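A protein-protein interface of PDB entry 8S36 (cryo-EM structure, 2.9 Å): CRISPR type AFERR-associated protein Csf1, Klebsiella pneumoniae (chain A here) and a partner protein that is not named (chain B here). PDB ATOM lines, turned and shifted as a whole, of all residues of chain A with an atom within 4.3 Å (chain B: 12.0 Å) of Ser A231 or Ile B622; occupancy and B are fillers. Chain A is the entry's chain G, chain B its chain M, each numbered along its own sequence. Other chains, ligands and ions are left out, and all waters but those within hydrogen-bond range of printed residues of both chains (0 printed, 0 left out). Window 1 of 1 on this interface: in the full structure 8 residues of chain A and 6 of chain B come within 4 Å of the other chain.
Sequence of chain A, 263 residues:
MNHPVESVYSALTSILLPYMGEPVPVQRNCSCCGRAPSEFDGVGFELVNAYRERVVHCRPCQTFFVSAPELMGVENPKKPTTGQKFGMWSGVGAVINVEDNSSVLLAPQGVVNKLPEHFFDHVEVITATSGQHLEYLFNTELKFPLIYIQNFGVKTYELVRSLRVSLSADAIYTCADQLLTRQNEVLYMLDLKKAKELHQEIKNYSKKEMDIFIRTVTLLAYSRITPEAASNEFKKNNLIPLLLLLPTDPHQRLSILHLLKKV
The side-chain hydroxyl (OG) of Ser A231 is in hydrogen-bond range of the side-chain carboxylate (OD1) of Asp B621 (3.4 Å). The side-chain amino group (NZ) of Lys A235 is in salt-bridge range of the side-chain carboxylate (OE1) of Glu B620, 3.3 Å away. OE2 of Glu A228 lies close to OE2 of Glu B619, at 3.0 Å.
OG of Ser A231 sits close to O of Pro A227 (3.4 Å). O of Glu A228 lies within hydrogen-bond range of OG of Ser A231. The backbone carbonyl oxygen (O) of Glu A228 sits close to the side-chain amide oxygen (OD1) of Asn A232 (2.9 Å). OG of Ser A231 lies within hydrogen-bond range of OD1 of Asn A232, at 3.4 Å. N of Ile B622 lies close to OE2 of Glu B620 (3.3 Å).
Pro A227 touches Gln B623. Tyr B617 touches Glu A228. Ser A231 touches Ile B622 (CB to N, 3.8 Å). Lys A235 touches Ile B622. Ile B622 touches Ile A240 (CD1 to CG2, 3.5 Å). CG2 of Ile B622 touches CD1 of Leu A243, at 3.3 Å.
Ile B622 touches just these residues of chain A: Ser A231 (3.8 Å), Lys A235 (3.7 Å), Ile A240 (3.5 Å) and Leu A243 (3.3 Å). Of chain B, only Gln B623 comes within 4 Å of Pro A227. Ala A229 touches none of the printed residues of chain B. No residue of chain B comes within 4 Å of Ala A230. No residue of chain B comes within 4 Å of Glu A233. No residue of chain B comes within 4 Å of Phe A234. Of chain B, only Glu B620 and Ile B622 come within 4 Å of Lys A235. Of chain B, only Ile B622 comes within 4 Å of Ile A240. Of chain B, only Ile B622 comes within 4 Å of Leu A243. Of the printed residues of chain A, Asp B621 touches Ser A231 (3.4 Å). Of the printed residues of chain A, Glu B619 touches Glu A228 (3.0 Å). Printed residues of chain A within 4 Å of Gln B623: Pro A227. Ala B616 touches none of the printed residues of chain A. The nearest printed residue of chain A that does not touch Glu B620 is Ser A231 (4.7 Å).
Of the 9 printed residues of chain B, 6 touch a printed residue of chain A. Hydrophobic or aromatic side chains of chain B within 4 Å of the printed part of chain A: Tyr B617 and Ile B622. Hydrophobic or aromatic side chains of chain A within 4 Å of the printed part of chain B: Pro A227, Ile A240 and Leu A243. Along chain A the printed residues that touch a printed residue of chain B span positions 227 to 243. Among the printed residues, 9 pairs touch across the chains. Among the printed residues, Asp or Glu carboxylates within 4 Å of a Lys or Arg side-chain nitrogen of the other chain: Lys A235 with Glu B620.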
ATOM      1  N   PRO A 227      29.286  29.879 -18.749  1.00  0.00           N
ATOM      2  CA  PRO A 227      28.841  29.003 -19.845  1.00  0.00           C
ATOM      3  C   PRO A 227      28.138  29.750 -20.958  1.00  0.00           C
ATOM      4  O   PRO A 227      28.244  29.349 -22.122  1.00  0.00           O
ATOM      5  CB  PRO A 227      27.902  28.017 -19.139  1.00  0.00           C
ATOM      6  CG  PRO A 227      28.422  27.959 -17.762  1.00  0.00           C
ATOM      7  CD  PRO A 227      28.834  29.365 -17.445  1.00  0.00           C
ATOM      8  N   GLU A 228      27.414  30.824 -20.639  1.00  0.00           N
ATOM      9  CA  GLU A 228      26.767  31.613 -21.680  1.00  0.00           C
ATOM     10  C   GLU A 228      27.802  32.229 -22.613  1.00  0.00           C
ATOM     11  O   GLU A 228      27.665  32.167 -23.841  1.00  0.00           O
ATOM     12  CB  GLU A 228      25.896  32.698 -21.044  1.00  0.00           C
ATOM     13  CG  GLU A 228      24.954  33.397 -22.018  1.00  0.00           C
ATOM     14  CD  GLU A 228      24.564  34.797 -21.572  1.00  0.00           C
ATOM     15  OE1 GLU A 228      25.038  35.250 -20.509  1.00  0.00           O
ATOM     16  OE2 GLU A 228      23.775  35.447 -22.290  1.00  0.00           O
ATOM     17  N   ALA A 229      28.849  32.831 -22.045  1.00  0.00           N
ATOM     18  CA  ALA A 229      29.894  33.424 -22.872  1.00  0.00           C
ATOM     19  C   ALA A 229      30.602  32.366 -23.707  1.00  0.00           C
ATOM     20  O   ALA A 229      30.882  32.585 -24.893  1.00  0.00           O
ATOM     21  CB  ALA A 229      30.897  34.168 -21.991  1.00  0.00           C
ATOM     22  N   ALA A 230      30.910  31.215 -23.106  1.00  0.00           N
ATOM     23  CA  ALA A 230      31.581  30.157 -23.852  1.00  0.00           C
ATOM     24  C   ALA A 230      30.709  29.656 -24.993  1.00  0.00           C
ATOM     25  O   ALA A 230      31.198  29.432 -26.105  1.00  0.00           O
ATOM     26  CB  ALA A 230      31.948  29.008 -22.915  1.00  0.00           C
ATOM     27  N   SER A 231      29.408  29.499 -24.744  1.00  0.00           N
ATOM     28  CA  SER A 231      28.502  29.061 -25.799  1.00  0.00           C
ATOM     29  C   SER A 231      28.418  30.101 -26.904  1.00  0.00           C
ATOM     30  O   SER A 231      28.356  29.757 -28.090  1.00  0.00           O
ATOM     31  CB  SER A 231      27.117  28.781 -25.218  1.00  0.00           C
ATOM     32  OG  SER A 231      26.434  29.989 -24.933  1.00  0.00           O
ATOM     33  N   ASN A 232      28.408  31.383 -26.533  1.00  0.00           N
ATOM     34  CA  ASN A 232      28.408  32.438 -27.540  1.00  0.00           C
ATOM     35  C   ASN A 232      29.655  32.362 -28.408  1.00  0.00           C
ATOM     36  O   ASN A 232      29.571  32.470 -29.636  1.00  0.00           O
ATOM     37  CB  ASN A 232      28.310  33.804 -26.864  1.00  0.00           C
ATOM     38  CG  ASN A 232      26.943  34.060 -26.264  1.00  0.00           C
ATOM     39  OD1 ASN A 232      26.134  33.143 -26.121  1.00  0.00           O
ATOM     40  ND2 ASN A 232      26.677  35.311 -25.907  1.00  0.00           N
ATOM     41  N   GLU A 233      30.822  32.172 -27.787  1.00  0.00           N
ATOM     42  CA  GLU A 233      32.056  32.063 -28.561  1.00  0.00           C
ATOM     43  C   GLU A 233      32.023  30.846 -29.477  1.00  0.00           C
ATOM     44  O   GLU A 233      32.417  30.928 -30.646  1.00  0.00           O
ATOM     45  CB  GLU A 233      33.268  31.987 -27.628  1.00  0.00           C
ATOM     46  CG  GLU A 233      33.449  33.163 -26.662  1.00  0.00           C
ATOM     47  CD  GLU A 233      32.739  34.429 -27.102  1.00  0.00           C
ATOM     48  OE1 GLU A 233      33.098  34.975 -28.167  1.00  0.00           O
ATOM     49  OE2 GLU A 233      31.820  34.878 -26.384  1.00  0.00           O
ATOM     50  N   PHE A 234      31.543  29.711 -28.966  1.00  0.00           N
ATOM     51  CA  PHE A 234      31.487  28.497 -29.776  1.00  0.00           C
ATOM     52  C   PHE A 234      30.562  28.682 -30.971  1.00  0.00           C
ATOM     53  O   PHE A 234      30.902  28.292 -32.095  1.00  0.00           O
ATOM     54  CB  PHE A 234      31.032  27.311 -28.923  1.00  0.00           C
ATOM     55  CG  PHE A 234      32.055  26.851 -27.914  1.00  0.00           C
ATOM     56  CD1 PHE A 234      33.363  26.597 -28.288  1.00  0.00           C
ATOM     57  CD2 PHE A 234      31.697  26.655 -26.592  1.00  0.00           C
ATOM     58  CE1 PHE A 234      34.295  26.171 -27.363  1.00  0.00           C
ATOM     59  CE2 PHE A 234      32.624  26.229 -25.662  1.00  0.00           C
ATOM     60  CZ  PHE A 234      33.924  25.986 -26.049  1.00  0.00           C
ATOM     61  N   LYS A 235      29.390  29.276 -30.751  1.00  0.00           N
ATOM     62  CA  LYS A 235      28.441  29.465 -31.841  1.00  0.00           C
ATOM     63  C   LYS A 235      28.961  30.479 -32.851  1.00  0.00           C
ATOM     64  O   LYS A 235      28.813  30.287 -34.064  1.00  0.00           O
ATOM     65  CB  LYS A 235      27.087  29.907 -31.285  1.00  0.00           C
ATOM     66  CG  LYS A 235      26.277  28.781 -30.663  1.00  0.00           C
ATOM     67  CD  LYS A 235      24.954  29.286 -30.109  1.00  0.00           C
ATOM     68  CE  LYS A 235      24.408  28.361 -29.030  1.00  0.00           C
ATOM     69  NZ  LYS A 235      24.510  26.924 -29.409  1.00  0.00           N
ATOM     70  N   ILE A 240      30.631  24.055 -32.585  1.00  0.00           N
ATOM     71  CA  ILE A 240      29.737  23.074 -31.966  1.00  0.00           C
ATOM     72  C   ILE A 240      30.138  21.643 -32.305  1.00  0.00           C
ATOM     73  O   ILE A 240      30.144  20.795 -31.396  1.00  0.00           O
ATOM     74  CB  ILE A 240      28.274  23.376 -32.345  1.00  0.00           C
ATOM     75  CG1 ILE A 240      27.912  24.857 -32.133  1.00  0.00           C
ATOM     76  CG2 ILE A 240      27.329  22.479 -31.554  1.00  0.00           C
ATOM     77  CD1 ILE A 240      27.977  25.347 -30.696  1.00  0.00           C
ATOM     78  N   LEU A 243      32.605  20.545 -29.981  1.00  0.00           N
ATOM     79  CA  LEU A 243      32.103  20.359 -28.625  1.00  0.00           C
ATOM     80  C   LEU A 243      31.378  19.036 -28.472  1.00  0.00           C
ATOM     81  O   LEU A 243      31.419  18.428 -27.396  1.00  0.00           O
ATOM     82  CB  LEU A 243      31.155  21.497 -28.248  1.00  0.00           C
ATOM     83  CG  LEU A 243      31.711  22.729 -27.538  1.00  0.00           C
ATOM     84  CD1 LEU A 243      30.574  23.710 -27.328  1.00  0.00           C
ATOM     85  CD2 LEU A 243      32.372  22.375 -26.210  1.00  0.00           C
ATOM     86  N   ALA B 616      15.812  36.751 -19.070  1.00  0.00           N
ATOM     87  CA  ALA B 616      17.189  36.938 -19.491  1.00  0.00           C
ATOM     88  C   ALA B 616      17.771  35.603 -19.922  1.00  0.00           C
ATOM     89  O   ALA B 616      17.303  34.538 -19.510  1.00  0.00           O
ATOM     90  CB  ALA B 616      18.041  37.540 -18.366  1.00  0.00           C
ATOM     91  N   TYR B 617      18.825  35.687 -20.727  1.00  0.00           N
ATOM     92  CA  TYR B 617      19.550  34.530 -21.252  1.00  0.00           C
ATOM     93  C   TYR B 617      18.579  33.425 -21.666  1.00  0.00           C
ATOM     94  O   TYR B 617      18.644  32.285 -21.205  1.00  0.00           O
ATOM     95  CB  TYR B 617      20.576  34.010 -20.238  1.00  0.00           C
ATOM     96  CG  TYR B 617      21.409  35.057 -19.502  1.00  0.00           C
ATOM     97  CD1 TYR B 617      21.551  36.357 -19.985  1.00  0.00           C
ATOM     98  CD2 TYR B 617      22.042  34.741 -18.306  1.00  0.00           C
ATOM     99  CE1 TYR B 617      22.302  37.297 -19.308  1.00  0.00           C
ATOM    100  CE2 TYR B 617      22.795  35.678 -17.623  1.00  0.00           C
ATOM    101  CZ  TYR B 617      22.921  36.954 -18.128  1.00  0.00           C
ATOM    102  OH  TYR B 617      23.669  37.890 -17.452  1.00  0.00           O
ATOM    103  N   PHE B 618      17.662  33.791 -22.562  1.00  0.00           N
ATOM    104  CA  PHE B 618      16.644  32.877 -23.063  1.00  0.00           C
ATOM    105  C   PHE B 618      17.109  32.104 -24.293  1.00  0.00           C
ATOM    106  O   PHE B 618      16.274  31.598 -25.050  1.00  0.00           O
ATOM    107  CB  PHE B 618      15.349  33.636 -23.374  1.00  0.00           C
ATOM    108  CG  PHE B 618      15.516  34.759 -24.360  1.00  0.00           C
ATOM    109  CD1 PHE B 618      15.459  34.518 -25.723  1.00  0.00           C
ATOM    110  CD2 PHE B 618      15.722  36.056 -23.923  1.00  0.00           C
ATOM    111  CE1 PHE B 618      15.610  35.548 -26.629  1.00  0.00           C
ATOM    112  CE2 PHE B 618      15.875  37.090 -24.825  1.00  0.00           C
ATOM    113  CZ  PHE B 618      15.818  36.836 -26.180  1.00  0.00           C
ATOM    114  N   GLU B 619      18.417  32.004 -24.500  1.00  0.00           N
ATOM    115  CA  GLU B 619      18.985  31.260 -25.612  1.00  0.00           C
ATOM    116  C   GLU B 619      19.284  29.835 -25.147  1.00  0.00           C
ATOM    117  O   GLU B 619      18.925  29.434 -24.037  1.00  0.00           O
ATOM    118  CB  GLU B 619      20.228  31.970 -26.155  1.00  0.00           C
ATOM    119  CG  GLU B 619      21.400  32.103 -25.173  1.00  0.00           C
ATOM    120  CD  GLU B 619      21.287  33.310 -24.253  1.00  0.00           C
ATOM    121  OE1 GLU B 619      20.563  34.268 -24.598  1.00  0.00           O
ATOM    122  OE2 GLU B 619      21.923  33.296 -23.179  1.00  0.00           O
ATOM    123  N   GLU B 620      19.948  29.056 -25.996  1.00  0.00           N
ATOM    124  CA  GLU B 620      20.303  27.677 -25.692  1.00  0.00           C
ATOM    125  C   GLU B 620      21.820  27.585 -25.616  1.00  0.00           C
ATOM    126  O   GLU B 620      22.516  27.928 -26.579  1.00  0.00           O
ATOM    127  CB  GLU B 620      19.748  26.722 -26.751  1.00  0.00           C
ATOM    128  CG  GLU B 620      20.415  25.346 -26.791  1.00  0.00           C
ATOM    129  CD  GLU B 620      21.588  25.276 -27.756  1.00  0.00           C
ATOM    130  OE1 GLU B 620      21.484  25.831 -28.870  1.00  0.00           O
ATOM    131  OE2 GLU B 620      22.617  24.666 -27.395  1.00  0.00           O
ATOM    132  N   ASP B 621      22.322  27.122 -24.477  1.00  0.00           N
ATOM    133  CA  ASP B 621      23.752  26.964 -24.261  1.00  0.00           C
ATOM    134  C   ASP B 621      24.173  25.578 -24.725  1.00  0.00           C
ATOM    135  O   ASP B 621      23.543  24.578 -24.366  1.00  0.00           O
ATOM    136  CB  ASP B 621      24.102  27.165 -22.787  1.00  0.00           C
ATOM    137  CG  ASP B 621      23.668  28.520 -22.266  1.00  0.00           C
ATOM    138  OD1 ASP B 621      23.622  29.477 -23.066  1.00  0.00           O
ATOM    139  OD2 ASP B 621      23.372  28.627 -21.058  1.00  0.00           O
ATOM    140  N   ILE B 622      25.242  25.521 -25.520  1.00  0.00           N
ATOM    141  CA  ILE B 622      25.651  24.251 -26.107  1.00  0.00           C
ATOM    142  C   ILE B 622      26.443  23.404 -25.122  1.00  0.00           C
ATOM    143  O   ILE B 622      26.488  22.176 -25.270  1.00  0.00           O
ATOM    144  CB  ILE B 622      26.463  24.495 -27.394  1.00  0.00           C
ATOM    145  CG1 ILE B 622      26.810  23.172 -28.092  1.00  0.00           C
ATOM    146  CG2 ILE B 622      27.733  25.303 -27.105  1.00  0.00           C
ATOM    147  CD1 ILE B 622      25.604  22.368 -28.539  1.00  0.00           C
ATOM    148  N   GLN B 623      27.061  24.019 -24.112  1.00  0.00           N
ATOM    149  CA  GLN B 623      27.725  23.269 -23.048  1.00  0.00           C
ATOM    150  C   GLN B 623      26.671  22.856 -22.021  1.00  0.00           C
ATOM    151  O   GLN B 623      26.551  23.415 -20.928  1.00  0.00           O
ATOM    152  CB  GLN B 623      28.837  24.097 -22.420  1.00  0.00           C
ATOM    153  CG  GLN B 623      29.628  23.347 -21.351  1.00  0.00           C
ATOM    154  CD  GLN B 623      29.320  23.796 -19.929  1.00  0.00           C
ATOM    155  OE1 GLN B 623      28.497  24.683 -19.701  1.00  0.00           O
ATOM    156  NE2 GLN B 623      29.987  23.178 -18.964  1.00  0.00           N
ATOM    157  N   CYS B 624      25.885  21.855 -22.404  1.00  0.00           N
ATOM    158  CA  CYS B 624      24.795  21.368 -21.570  1.00  0.00           C
ATOM    159  C   CYS B 624      25.299  20.346 -20.559  1.00  0.00           C
ATOM    160  O   CYS B 624      26.241  19.603 -20.831  1.00  0.00           O
ATOM    161  CB  CYS B 624      23.696  20.749 -22.436  1.00  0.00           C
ATOM    162  SG  CYS B 624      22.062  20.742 -21.669  1.00  0.00           S
